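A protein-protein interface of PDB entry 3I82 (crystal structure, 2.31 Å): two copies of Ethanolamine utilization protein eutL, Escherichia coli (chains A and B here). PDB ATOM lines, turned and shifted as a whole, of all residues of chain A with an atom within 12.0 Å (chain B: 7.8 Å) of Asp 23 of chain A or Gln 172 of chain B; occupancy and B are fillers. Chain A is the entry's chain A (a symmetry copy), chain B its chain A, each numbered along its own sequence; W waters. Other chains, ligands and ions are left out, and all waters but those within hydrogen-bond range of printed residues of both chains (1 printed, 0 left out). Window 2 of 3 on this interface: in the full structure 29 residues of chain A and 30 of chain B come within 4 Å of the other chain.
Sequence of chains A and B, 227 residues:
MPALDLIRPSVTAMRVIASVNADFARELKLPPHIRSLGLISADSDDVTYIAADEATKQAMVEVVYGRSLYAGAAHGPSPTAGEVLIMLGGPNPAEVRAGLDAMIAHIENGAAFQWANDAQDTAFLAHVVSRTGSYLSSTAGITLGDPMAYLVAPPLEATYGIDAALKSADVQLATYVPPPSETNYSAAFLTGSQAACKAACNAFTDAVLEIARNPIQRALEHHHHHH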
ATOM      1  N   ILE A  17       7.848 -11.980  -8.821  1.00  0.00           N
ATOM      2  CA  ILE A  17       8.231 -11.512  -7.507  1.00  0.00           C
ATOM      3  C   ILE A  17       8.557 -12.797  -6.757  1.00  0.00           C
ATOM      4  O   ILE A  17       7.666 -13.554  -6.375  1.00  0.00           O
ATOM      5  CB  ILE A  17       7.076 -10.768  -6.800  1.00  0.00           C
ATOM      6  CG1 ILE A  17       6.572  -9.610  -7.669  1.00  0.00           C
ATOM      7  CG2 ILE A  17       7.545 -10.259  -5.453  1.00  0.00           C
ATOM      8  CD1 ILE A  17       5.506  -8.749  -6.994  1.00  0.00           C
ATOM      9  N   SER A  19       9.738 -13.295  -3.771  1.00  0.00           N
ATOM     10  CA  SER A  19       9.283 -13.287  -2.383  1.00  0.00           C
ATOM     11  C   SER A  19       8.484 -12.022  -2.110  1.00  0.00           C
ATOM     12  O   SER A  19       9.056 -10.944  -1.911  1.00  0.00           O
ATOM     13  CB  SER A  19      10.478 -13.355  -1.431  1.00  0.00           C
ATOM     14  OG  SER A  19      10.050 -13.331  -0.084  1.00  0.00           O
ATOM     15  N   VAL A  20       7.163 -12.168  -2.089  1.00  0.00           N
ATOM     16  CA  VAL A  20       6.264 -11.047  -1.880  1.00  0.00           C
ATOM     17  C   VAL A  20       6.425 -10.427  -0.502  1.00  0.00           C
ATOM     18  O   VAL A  20       6.561 -11.135   0.498  1.00  0.00           O
ATOM     19  CB  VAL A  20       4.789 -11.473  -2.051  1.00  0.00           C
ATOM     20  CG1 VAL A  20       3.871 -10.248  -1.994  1.00  0.00           C
ATOM     21  CG2 VAL A  20       4.606 -12.192  -3.364  1.00  0.00           C
ATOM     22  N   ASN A  21       6.407  -9.098  -0.460  1.00  0.00           N
ATOM     23  CA  ASN A  21       6.505  -8.363   0.796  1.00  0.00           C
ATOM     24  C   ASN A  21       5.371  -8.798   1.715  1.00  0.00           C
ATOM     25  O   ASN A  21       4.241  -9.003   1.258  1.00  0.00           O
ATOM     26  CB  ASN A  21       6.411  -6.864   0.537  1.00  0.00           C
ATOM     27  CG  ASN A  21       6.312  -6.059   1.820  1.00  0.00           C
ATOM     28  OD1 ASN A  21       5.216  -5.710   2.258  1.00  0.00           O
ATOM     29  ND2 ASN A  21       7.460  -5.770   2.435  1.00  0.00           N
ATOM     30  N   ALA A  22       5.678  -8.949   3.001  1.00  0.00           N
ATOM     31  CA  ALA A  22       4.698  -9.402   3.985  1.00  0.00           C
ATOM     32  C   ALA A  22       3.445  -8.536   4.001  1.00  0.00           C
ATOM     33  O   ALA A  22       2.338  -9.047   3.848  1.00  0.00           O
ATOM     34  CB  ALA A  22       5.323  -9.439   5.366  1.00  0.00           C
ATOM     35  N   ASP A  23       3.633  -7.231   4.175  1.00  0.00           N
ATOM     36  CA  ASP A  23       2.526  -6.270   4.243  1.00  0.00           C
ATOM     37  C   ASP A  23       1.589  -6.388   3.038  1.00  0.00           C
ATOM     38  O   ASP A  23       0.377  -6.575   3.189  1.00  0.00           O
ATOM     39  CB  ASP A  23       3.086  -4.845   4.337  1.00  0.00           C
ATOM     40  CG  ASP A  23       2.015  -3.804   4.624  1.00  0.00           C
ATOM     41  OD1 ASP A  23       0.816  -4.156   4.707  1.00  0.00           O
ATOM     42  OD2 ASP A  23       2.379  -2.616   4.771  1.00  0.00           O
ATOM     43  N   PHE A  24       2.176  -6.279   1.850  1.00  0.00           N
ATOM     44  CA  PHE A  24       1.450  -6.398   0.582  1.00  0.00           C
ATOM     45  C   PHE A  24       0.765  -7.764   0.484  1.00  0.00           C
ATOM     46  O   PHE A  24      -0.349  -7.874  -0.036  1.00  0.00           O
ATOM     47  CB  PHE A  24       2.436  -6.217  -0.589  1.00  0.00           C
ATOM     48  CG  PHE A  24       1.792  -5.892  -1.924  1.00  0.00           C
ATOM     49  CD1 PHE A  24       0.568  -5.228  -2.003  1.00  0.00           C
ATOM     50  CD2 PHE A  24       2.464  -6.183  -3.105  1.00  0.00           C
ATOM     51  CE1 PHE A  24       0.024  -4.880  -3.237  1.00  0.00           C
ATOM     52  CE2 PHE A  24       1.928  -5.838  -4.340  1.00  0.00           C
ATOM     53  CZ  PHE A  24       0.705  -5.186  -4.408  1.00  0.00           C
ATOM     54  N   ALA A  25       1.429  -8.801   0.996  1.00  0.00           N
ATOM     55  CA  ALA A  25       0.876 -10.156   0.975  1.00  0.00           C
ATOM     56  C   ALA A  25      -0.405 -10.206   1.787  1.00  0.00           C
ATOM     57  O   ALA A  25      -1.389 -10.832   1.377  1.00  0.00           O
ATOM     58  CB  ALA A  25       1.876 -11.142   1.529  1.00  0.00           C
ATOM     59  N   ARG A  26      -0.405  -9.517   2.927  1.00  0.00           N
ATOM     60  CA  ARG A  26      -1.592  -9.470   3.779  1.00  0.00           C
ATOM     61  C   ARG A  26      -2.735  -8.754   3.068  1.00  0.00           C
ATOM     62  O   ARG A  26      -3.858  -9.257   3.040  1.00  0.00           O
ATOM     63  CB  ARG A  26      -1.283  -8.778   5.103  1.00  0.00           C
ATOM     64  CG  ARG A  26      -0.250  -9.517   5.923  1.00  0.00           C
ATOM     65  CD  ARG A  26       0.113  -8.765   7.178  1.00  0.00           C
ATOM     66  NE  ARG A  26       1.381  -9.236   7.727  1.00  0.00           N
ATOM     67  CZ  ARG A  26       2.433  -8.459   7.961  1.00  0.00           C
ATOM     68  NH1 ARG A  26       2.366  -7.148   7.744  1.00  0.00           N
ATOM     69  NH2 ARG A  26       3.546  -8.989   8.451  1.00  0.00           N
ATOM     70  N   GLU A  27      -2.446  -7.590   2.490  1.00  0.00           N
ATOM     71  CA  GLU A  27      -3.456  -6.839   1.748  1.00  0.00           C
ATOM     72  C   GLU A  27      -4.014  -7.647   0.573  1.00  0.00           C
ATOM     73  O   GLU A  27      -5.183  -7.519   0.232  1.00  0.00           O
ATOM     74  CB  GLU A  27      -2.885  -5.510   1.248  1.00  0.00           C
ATOM     75  CG  GLU A  27      -3.266  -4.314   2.112  1.00  0.00           C
ATOM     76  CD  GLU A  27      -4.725  -3.924   1.955  1.00  0.00           C
ATOM     77  OE1 GLU A  27      -5.165  -3.729   0.803  1.00  0.00           O
ATOM     78  OE2 GLU A  27      -5.426  -3.809   2.982  1.00  0.00           O
ATOM     79  N   LEU A  28      -3.174  -8.481  -0.036  1.00  0.00           N
ATOM     80  CA  LEU A  28      -3.591  -9.335  -1.153  1.00  0.00           C
ATOM     81  C   LEU A  28      -4.277 -10.614  -0.666  1.00  0.00           C
ATOM     82  O   LEU A  28      -4.839 -11.367  -1.462  1.00  0.00           O
ATOM     83  CB  LEU A  28      -2.382  -9.699  -2.015  1.00  0.00           C
ATOM     84  CG  LEU A  28      -1.760  -8.571  -2.843  1.00  0.00           C
ATOM     85  CD1 LEU A  28      -0.514  -9.076  -3.553  1.00  0.00           C
ATOM     86  CD2 LEU A  28      -2.773  -8.036  -3.846  1.00  0.00           C
ATOM     87  N   LYS A  29      -4.203 -10.852   0.643  1.00  0.00           N
ATOM     88  CA  LYS A  29      -4.836 -11.991   1.305  1.00  0.00           C
ATOM     89  C   LYS A  29      -4.308 -13.312   0.787  1.00  0.00           C
ATOM     90  O   LYS A  29      -5.069 -14.249   0.524  1.00  0.00           O
ATOM     91  CB  LYS A  29      -6.356 -11.898   1.168  1.00  0.00           C
ATOM     92  CG  LYS A  29      -6.880 -10.577   1.703  1.00  0.00           C
ATOM     93  CD  LYS A  29      -8.316 -10.642   2.188  1.00  0.00           C
ATOM     94  CE  LYS A  29      -8.654  -9.371   2.967  1.00  0.00           C
ATOM     95  NZ  LYS A  29     -10.004  -9.403   3.591  1.00  0.00           N
ATOM     96  N   LEU A  30      -2.991 -13.380   0.648  1.00  0.00           N
ATOM     97  CA  LEU A  30      -2.346 -14.587   0.146  1.00  0.00           C
ATOM     98  C   LEU A  30      -2.325 -15.710   1.180  1.00  0.00           C
ATOM     99  O   LEU A  30      -2.058 -15.486   2.368  1.00  0.00           O
ATOM    100  CB  LEU A  30      -0.922 -14.282  -0.311  1.00  0.00           C
ATOM    101  CG  LEU A  30      -0.730 -13.235  -1.415  1.00  0.00           C
ATOM    102  CD1 LEU A  30       0.756 -13.070  -1.719  1.00  0.00           C
ATOM    103  CD2 LEU A  30      -1.502 -13.626  -2.677  1.00  0.00           C
ATOM    104  N   PRO A  31      -2.599 -16.950   0.742  1.00  0.00           N
ATOM    105  CA  PRO A  31      -2.535 -18.028   1.722  1.00  0.00           C
ATOM    106  C   PRO A  31      -1.095 -18.161   2.231  1.00  0.00           C
ATOM    107  O   PRO A  31      -0.156 -17.654   1.604  1.00  0.00           O
ATOM    108  CB  PRO A  31      -2.981 -19.254   0.919  1.00  0.00           C
ATOM    109  CG  PRO A  31      -3.884 -18.662  -0.143  1.00  0.00           C
ATOM    110  CD  PRO A  31      -3.101 -17.444  -0.554  1.00  0.00           C
ATOM    111  N   ILE A  34       1.448 -19.560  -0.266  1.00  0.00           N
ATOM    112  CA  ILE A  34       1.770 -18.739  -1.436  1.00  0.00           C
ATOM    113  C   ILE A  34       2.531 -17.457  -1.113  1.00  0.00           C
ATOM    114  O   ILE A  34       1.940 -16.458  -0.699  1.00  0.00           O
ATOM    115  CB  ILE A  34       0.504 -18.381  -2.252  1.00  0.00           C
ATOM    116  CG1 ILE A  34      -0.054 -19.639  -2.908  1.00  0.00           C
ATOM    117  CG2 ILE A  34       0.829 -17.350  -3.330  1.00  0.00           C
ATOM    118  CD1 ILE A  34      -1.065 -19.360  -3.980  1.00  0.00           C
ATOM    119  N   ARG A  35       3.843 -17.492  -1.331  1.00  0.00           N
ATOM    120  CA  ARG A  35       4.674 -16.315  -1.103  1.00  0.00           C
ATOM    121  C   ARG A  35       5.513 -15.905  -2.321  1.00  0.00           C
ATOM    122  O   ARG A  35       6.314 -14.975  -2.239  1.00  0.00           O
ATOM    123  CB  ARG A  35       5.553 -16.519   0.138  1.00  0.00           C
ATOM    124  CG  ARG A  35       4.790 -16.403   1.480  1.00  0.00           C
ATOM    125  CD  ARG A  35       4.156 -15.016   1.690  1.00  0.00           C
ATOM    126  NE  ARG A  35       2.695 -15.069   1.805  1.00  0.00           N
ATOM    127  CZ  ARG A  35       2.020 -15.093   2.955  1.00  0.00           C
ATOM    128  NH1 ARG A  35       2.652 -15.061   4.124  1.00  0.00           N
ATOM    129  NH2 ARG A  35       0.696 -15.129   2.939  1.00  0.00           N
ATOM    130  N   LEU A  37       5.019 -14.797  -6.442  1.00  0.00           N
ATOM    131  CA  LEU A  37       3.937 -14.269  -7.260  1.00  0.00           C
ATOM    132  C   LEU A  37       4.368 -13.913  -8.677  1.00  0.00           C
ATOM    133  O   LEU A  37       5.301 -13.143  -8.870  1.00  0.00           O
ATOM    134  CB  LEU A  37       3.356 -13.034  -6.568  1.00  0.00           C
ATOM    135  CG  LEU A  37       1.927 -12.583  -6.852  1.00  0.00           C
ATOM    136  CD1 LEU A  37       0.926 -13.508  -6.182  1.00  0.00           C
ATOM    137  CD2 LEU A  37       1.750 -11.158  -6.329  1.00  0.00           C
ATOM    138  N   VAL A  64      -4.387 -15.667  -7.936  1.00  0.00           N
ATOM    139  CA  VAL A  64      -4.572 -14.752  -6.826  1.00  0.00           C
ATOM    140  C   VAL A  64      -5.462 -13.591  -7.246  1.00  0.00           C
ATOM    141  O   VAL A  64      -6.302 -13.131  -6.468  1.00  0.00           O
ATOM    142  CB  VAL A  64      -3.214 -14.190  -6.355  1.00  0.00           C
ATOM    143  CG1 VAL A  64      -3.423 -12.973  -5.453  1.00  0.00           C
ATOM    144  CG2 VAL A  64      -2.419 -15.278  -5.644  1.00  0.00           C
ATOM    145  N   MET A  87      -2.405 -12.452 -11.729  1.00  0.00           N
ATOM    146  CA  MET A  87      -1.410 -12.671 -10.685  1.00  0.00           C
ATOM    147  C   MET A  87      -1.556 -14.133 -10.287  1.00  0.00           C
ATOM    148  O   MET A  87      -2.595 -14.497  -9.737  1.00  0.00           O
ATOM    149  CB  MET A  87      -1.666 -11.798  -9.452  1.00  0.00           C
ATOM    150  CG  MET A  87      -1.567 -10.299  -9.670  1.00  0.00           C
ATOM    151  SD  MET A  87      -1.721  -9.477  -8.069  1.00  0.00           S
ATOM    152  CE  MET A  87      -2.506  -7.896  -8.514  1.00  0.00           C
ATOM    153  N   GLY B 141      -6.864   4.571   7.354  1.00  0.00           N
ATOM    154  CA  GLY B 141      -5.443   4.320   7.550  1.00  0.00           C
ATOM    155  C   GLY B 141      -4.621   5.589   7.454  1.00  0.00           C
ATOM    156  O   GLY B 141      -3.446   5.604   7.832  1.00  0.00           O
ATOM    157  N   MET B 148       2.228  11.025   3.187  1.00  0.00           N
ATOM    158  CA  MET B 148       1.947   9.814   2.437  1.00  0.00           C
ATOM    159  C   MET B 148       2.539   9.858   1.042  1.00  0.00           C
ATOM    160  O   MET B 148       2.842  10.928   0.511  1.00  0.00           O
ATOM    161  CB  MET B 148       0.439   9.542   2.341  1.00  0.00           C
ATOM    162  CG  MET B 148      -0.376  10.614   1.661  1.00  0.00           C
ATOM    163  SD  MET B 148      -1.685   9.898   0.648  1.00  0.00           S
ATOM    164  CE  MET B 148      -0.850   9.824  -0.921  1.00  0.00           C
ATOM    165  N   ALA B 149       2.754   8.671   0.480  1.00  0.00           N
ATOM    166  CA  ALA B 149       3.239   8.525  -0.889  1.00  0.00           C
ATOM    167  C   ALA B 149       2.038   8.110  -1.721  1.00  0.00           C
ATOM    168  O   ALA B 149       1.302   7.214  -1.333  1.00  0.00           O
ATOM    169  CB  ALA B 149       4.314   7.459  -0.972  1.00  0.00           C
ATOM    170  N   ILE B 162       4.648  -1.489  -6.173  1.00  0.00           N
ATOM    171  CA  ILE B 162       4.151  -1.379  -4.802  1.00  0.00           C
ATOM    172  C   ILE B 162       4.967  -2.295  -3.907  1.00  0.00           C
ATOM    173  O   ILE B 162       5.457  -1.872  -2.856  1.00  0.00           O
ATOM    174  CB  ILE B 162       2.657  -1.735  -4.687  1.00  0.00           C
ATOM    175  CG1 ILE B 162       1.806  -0.585  -5.239  1.00  0.00           C
ATOM    176  CG2 ILE B 162       2.281  -1.984  -3.233  1.00  0.00           C
ATOM    177  CD1 ILE B 162       0.328  -0.940  -5.422  1.00  0.00           C
ATOM    178  N   ASP B 163       5.118  -3.544  -4.337  1.00  0.00           N
ATOM    179  CA  ASP B 163       5.939  -4.521  -3.613  1.00  0.00           C
ATOM    180  C   ASP B 163       7.362  -3.972  -3.432  1.00  0.00           C
ATOM    181  O   ASP B 163       7.925  -4.011  -2.331  1.00  0.00           O
ATOM    182  CB  ASP B 163       5.986  -5.843  -4.395  1.00  0.00           C
ATOM    183  CG  ASP B 163       6.989  -6.837  -3.820  1.00  0.00           C
ATOM    184  OD1 ASP B 163       6.686  -7.455  -2.772  1.00  0.00           O
ATOM    185  OD2 ASP B 163       8.077  -7.001  -4.433  1.00  0.00           O
ATOM    186  N   ALA B 165       8.359  -0.925  -3.373  1.00  0.00           N
ATOM    187  CA  ALA B 165       8.404   0.268  -2.528  1.00  0.00           C
ATOM    188  C   ALA B 165       8.382  -0.121  -1.064  1.00  0.00           C
ATOM    189  O   ALA B 165       9.097   0.449  -0.240  1.00  0.00           O
ATOM    190  CB  ALA B 165       7.205   1.171  -2.829  1.00  0.00           C
ATOM    191  N   LEU B 166       7.526  -1.083  -0.758  1.00  0.00           N
ATOM    192  CA  LEU B 166       7.349  -1.593   0.605  1.00  0.00           C
ATOM    193  C   LEU B 166       8.606  -2.267   1.117  1.00  0.00           C
ATOM    194  O   LEU B 166       8.780  -2.385   2.319  1.00  0.00           O
ATOM    195  CB  LEU B 166       6.154  -2.565   0.637  1.00  0.00           C
ATOM    196  CG  LEU B 166       4.799  -1.851   0.489  1.00  0.00           C
ATOM    197  CD1 LEU B 166       3.722  -2.807   0.025  1.00  0.00           C
ATOM    198  CD2 LEU B 166       4.402  -1.177   1.803  1.00  0.00           C
ATOM    199  N   ALA B 169      11.610   1.051   1.869  1.00  0.00           N
ATOM    200  CA  ALA B 169      11.600   2.003   2.976  1.00  0.00           C
ATOM    201  C   ALA B 169      10.677   1.609   4.116  1.00  0.00           C
ATOM    202  O   ALA B 169       9.855   0.702   4.012  1.00  0.00           O
ATOM    203  CB  ALA B 169      11.242   3.394   2.462  1.00  0.00           C
ATOM    204  N   ASP B 170      10.821   2.317   5.230  1.00  0.00           N
ATOM    205  CA  ASP B 170       9.999   2.052   6.407  1.00  0.00           C
ATOM    206  C   ASP B 170       8.617   2.656   6.154  1.00  0.00           C
ATOM    207  O   ASP B 170       8.359   3.811   6.501  1.00  0.00           O
ATOM    208  CB  ASP B 170      10.669   2.652   7.667  1.00  0.00           C
ATOM    209  CG  ASP B 170       9.992   2.222   8.968  1.00  0.00           C
ATOM    210  OD1 ASP B 170       9.271   1.197   8.974  1.00  0.00           O
ATOM    211  OD2 ASP B 170      10.200   2.913   9.996  1.00  0.00           O
ATOM    212  N   VAL B 171       7.746   1.867   5.516  1.00  0.00           N
ATOM    213  CA  VAL B 171       6.406   2.327   5.177  1.00  0.00           C
ATOM    214  C   VAL B 171       5.366   1.226   5.276  1.00  0.00           C
ATOM    215  O   VAL B 171       5.683   0.034   5.254  1.00  0.00           O
ATOM    216  CB  VAL B 171       6.347   2.926   3.746  1.00  0.00           C
ATOM    217  CG1 VAL B 171       7.159   4.212   3.676  1.00  0.00           C
ATOM    218  CG2 VAL B 171       6.852   1.913   2.724  1.00  0.00           C
ATOM    219  N   GLN B 172       4.115   1.659   5.372  1.00  0.00           N
ATOM    220  CA  GLN B 172       2.969   0.768   5.475  1.00  0.00           C
ATOM    221  C   GLN B 172       1.988   1.018   4.338  1.00  0.00           C
ATOM    222  O   GLN B 172       1.874   2.136   3.839  1.00  0.00           O
ATOM    223  CB  GLN B 172       2.236   0.982   6.804  1.00  0.00           C
ATOM    224  CG  GLN B 172       2.941   0.449   8.033  1.00  0.00           C
ATOM    225  CD  GLN B 172       2.152   0.728   9.301  1.00  0.00           C
ATOM    226  OE1 GLN B 172       1.877   1.884   9.633  1.00  0.00           O
ATOM    227  NE2 GLN B 172       1.782  -0.332  10.016  1.00  0.00           N
ATOM    228  N   LEU B 173       1.278  -0.031   3.947  1.00  0.00           N
ATOM    229  CA  LEU B 173       0.265   0.065   2.905  1.00  0.00           C
ATOM    230  C   LEU B 173      -1.022   0.569   3.564  1.00  0.00           C
ATOM    231  O   LEU B 173      -1.654  -0.151   4.333  1.00  0.00           O
ATOM    232  CB  LEU B 173       0.044  -1.311   2.267  1.00  0.00           C
ATOM    233  CG  LEU B 173      -0.763  -1.417   0.975  1.00  0.00           C
ATOM    234  CD1 LEU B 173      -0.225  -0.470  -0.104  1.00  0.00           C
ATOM    235  CD2 LEU B 173      -0.706  -2.848   0.485  1.00  0.00           C
ATOM    236  N   ALA B 174      -1.391   1.815   3.282  1.00  0.00           N
ATOM    237  CA  ALA B 174      -2.596   2.397   3.869  1.00  0.00           C
ATOM    238  C   ALA B 174      -3.818   2.025   3.047  1.00  0.00           C
ATOM    239  O   ALA B 174      -4.819   1.524   3.572  1.00  0.00           O
ATOM    240  CB  ALA B 174      -2.461   3.909   3.957  1.00  0.00           C
ATOM    241  N   THR B 175      -3.737   2.286   1.749  1.00  0.00           N
ATOM    242  CA  THR B 175      -4.841   1.958   0.863  1.00  0.00           C
ATOM    243  C   THR B 175      -4.309   1.387  -0.422  1.00  0.00           C
ATOM    244  O   THR B 175      -3.355   1.908  -0.989  1.00  0.00           O
ATOM    245  CB  THR B 175      -5.701   3.188   0.515  1.00  0.00           C
ATOM    246  OG1 THR B 175      -5.246   3.779  -0.717  1.00  0.00           O
ATOM    247  CG2 THR B 175      -5.617   4.214   1.627  1.00  0.00           C
ATOM    248  N   ALA B 188      -1.773   3.148  -4.999  1.00  0.00           N
ATOM    249  CA  ALA B 188      -1.485   2.854  -3.611  1.00  0.00           C
ATOM    250  C   ALA B 188      -1.128   4.116  -2.832  1.00  0.00           C
ATOM    251  O   ALA B 188      -0.464   5.029  -3.341  1.00  0.00           O
ATOM    252  CB  ALA B 188      -0.345   1.843  -3.515  1.00  0.00           C
ATOM    253  N   PHE B 189      -1.604   4.168  -1.593  1.00  0.00           N
ATOM    254  CA  PHE B 189      -1.260   5.250  -0.678  1.00  0.00           C
ATOM    255  C   PHE B 189      -0.461   4.607   0.440  1.00  0.00           C
ATOM    256  O   PHE B 189      -1.021   3.802   1.194  1.00  0.00           O
ATOM    257  CB  PHE B 189      -2.501   5.910  -0.069  1.00  0.00           C
ATOM    258  CG  PHE B 189      -3.362   6.658  -1.053  1.00  0.00           C
ATOM    259  CD1 PHE B 189      -2.907   6.986  -2.321  1.00  0.00           C
ATOM    260  CD2 PHE B 189      -4.630   7.078  -0.672  1.00  0.00           C
ATOM    261  CE1 PHE B 189      -3.701   7.697  -3.192  1.00  0.00           C
ATOM    262  CE2 PHE B 189      -5.437   7.800  -1.542  1.00  0.00           C
ATOM    263  CZ  PHE B 189      -4.967   8.110  -2.807  1.00  0.00           C
ATOM    264  N   LEU B 190       0.829   4.948   0.510  1.00  0.00           N
ATOM    265  CA  LEU B 190       1.739   4.438   1.539  1.00  0.00           C
ATOM    266  C   LEU B 190       1.940   5.459   2.634  1.00  0.00           C
ATOM    267  O   LEU B 190       1.989   6.661   2.376  1.00  0.00           O
ATOM    268  CB  LEU B 190       3.113   4.093   0.964  1.00  0.00           C
ATOM    269  CG  LEU B 190       3.194   3.049  -0.143  1.00  0.00           C
ATOM    270  CD1 LEU B 190       4.640   2.613  -0.305  1.00  0.00           C
ATOM    271  CD2 LEU B 190       2.289   1.868   0.182  1.00  0.00           C
ATOM    272  N   THR B 191       2.120   4.956   3.844  1.00  0.00           N
ATOM    273  CA  THR B 191       2.242   5.797   5.017  1.00  0.00           C
ATOM    274  C   THR B 191       3.542   5.563   5.757  1.00  0.00           C
ATOM    275  O   THR B 191       4.162   4.516   5.632  1.00  0.00           O
ATOM    276  CB  THR B 191       1.028   5.558   5.958  1.00  0.00           C
ATOM    277  OG1 THR B 191       0.287   6.774   6.070  1.00  0.00           O
ATOM    278  CG2 THR B 191       1.454   5.117   7.340  1.00  0.00           C
ATOM    279  N   GLY B 192       3.927   6.537   6.559  1.00  0.00           N
ATOM    280  CA  GLY B 192       5.145   6.448   7.328  1.00  0.00           C
ATOM    281  C   GLY B 192       5.752   7.826   7.372  1.00  0.00           C
ATOM    282  O   GLY B 192       5.070   8.818   7.120  1.00  0.00           O
ATOM    283  N   SER B 193       7.032   7.885   7.708  1.00  0.00           N
ATOM    284  CA  SER B 193       7.798   9.144   7.746  1.00  0.00           C
ATOM    285  C   SER B 193       7.844   9.793   6.362  1.00  0.00           C
ATOM    286  O   SER B 193       7.655   9.115   5.352  1.00  0.00           O
ATOM    287  CB  SER B 193       9.240   8.875   8.208  1.00  0.00           C
ATOM    288  OG  SER B 193      10.162   9.498   7.316  1.00  0.00           O
ATOM    289  N   ALA B 196      10.879   8.537   4.409  1.00  0.00           N
ATOM    290  CA  ALA B 196      10.551   7.165   4.019  1.00  0.00           C
ATOM    291  C   ALA B 196       9.610   7.129   2.806  1.00  0.00           C
ATOM    292  O   ALA B 196       9.774   6.292   1.915  1.00  0.00           O
ATOM    293  CB  ALA B 196       9.911   6.424   5.187  1.00  0.00           C
ATOM    294  N   CYS B 197       8.642   8.044   2.769  1.00  0.00           N
ATOM    295  CA  CYS B 197       7.703   8.103   1.647  1.00  0.00           C
ATOM    296  C   CYS B 197       8.436   8.457   0.361  1.00  0.00           C
ATOM    297  O   CYS B 197       8.149   7.881  -0.698  1.00  0.00           O
ATOM    298  CB  CYS B 197       6.591   9.117   1.913  1.00  0.00           C
ATOM    299  SG  CYS B 197       5.489   8.627   3.265  1.00  0.00           S
ATOM    300  N   ALA B 200      10.160   5.405  -0.842  1.00  0.00           N
ATOM    301  CA  ALA B 200       9.168   4.562  -1.496  1.00  0.00           C
ATOM    302  C   ALA B 200       8.886   5.045  -2.915  1.00  0.00           C
ATOM    303  O   ALA B 200       8.774   4.232  -3.834  1.00  0.00           O
ATOM    304  CB  ALA B 200       7.878   4.536  -0.681  1.00  0.00           C
HETATM  305  O   HOH W   1       1.389  -2.162   7.187  1.00  0.00           O
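N of Asn 21 of chain A is in hydrogen-bond range of OD1 of Asp 163 of chain B (2.9 Å).
OD2 of Asp 23 of chain A is in hydrogen-bond range of N of Leu 173 of chain B (2.9 Å).
The backbone carbonyl oxygen of Arg 35 of chain A sits at hydrogen-bond distance from the backbone NH of Val 20 of chain A, at 2.9 Å.
The backbone carbonyl oxygen (O) of Gln 172 of chain B is in hydrogen-bond range of the backbone NH (N) of Thr 191 of chain B, 2.8 Å away.
The backbone NH (N) of Asp 23 of chain A sits at hydrogen-bond distance from the side-chain amide oxygen (OD1) of Asn 21 of chain A (2.9 Å).
OD1 of Asn 21 of chain A lies within hydrogen-bond range of N of Phe 24 of chain A (3.1 Å).
Asp 163 of chain B touches Ile 17 of chain A (OD2 to CG2, 3.5 Å).
Val 20 of chain A touches Asp 163 of chain B.
Asn 21 of chain A touches Leu 166 of chain B (ND2 to O, 3.6 Å).
Asp 23 of chain A touches Leu 166 of chain B.
Asp 23 of chain A touches Gln 172 of chain B (OD2 to CA, 3.5 Å).
Asp 163 of chain B touches Phe 24 of chain A.
Phe 24 of chain A touches Leu 166 of chain B (CB to CD1, 3.7 Å).
CD1 of Phe 24 of chain A touches CD2 of Leu 173 of chain B, 3.7 Å away.
Glu 27 of chain A touches Leu 173 of chain B.
Of chain B, only Leu 166, Gln 172 and Leu 173 come within 4 Å of Asp 23 of chain A.
Gln 172 of chain B touches just one residue of chain A: Asp 23.
No residue of chain B comes within 4 Å of Ala 22 of chain A.
Leu 166 of chain B touches just these residues of chain A: Asn 21 (3.6 Å), Asp 23 (3.9 Å) and Phe 24 (3.7 Å).
No residue of chain A comes within 4 Å of Ala 174 of chain B.
No residue of chain A comes within 4 Å of Leu 190 of chain B.
Printed residues of chain A within 4 Å of Asp 163 of chain B: Ile 17 (3.5 Å), Val 20 (3.7 Å), Asn 21 (2.9 Å) and Phe 24 (3.8 Å).
Of the printed residues of chain B, Ile 17 of chain A touches Asp 163 (3.5 Å).
Printed residues of chain A within 4 Å of Ile 162 of chain B: Phe 24 (3.7 Å).
Phe 189 of chain B touches none of the printed residues of chain A.
Arg 26 of chain A touches none of the printed residues of chain B.
Hydrophobic or aromatic side chains of chain A within 4 Å of the printed part of chain B: Ile 17 and Phe 24.
Along chain A the printed residues that touch a printed residue of chain B span positions 17 to 27.
Of the 23 printed residues of chain B, 5 touch a printed residue of chain A.
Hydrophobic or aromatic side chains of chain B within 4 Å of the printed part of chain A: Ile 162, Leu 166 and Leu 173.
No position is printed for both chains.
Of the 12 pairs that touch across the chains among the printed residues, none has its exchanged pair printed and touching as well.
Water W1 lies within hydrogen-bond range of OD2 of Asp 23 of chain A (2.7 Å) and NE2 of Gln 172 of chain B (3.4 Å).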
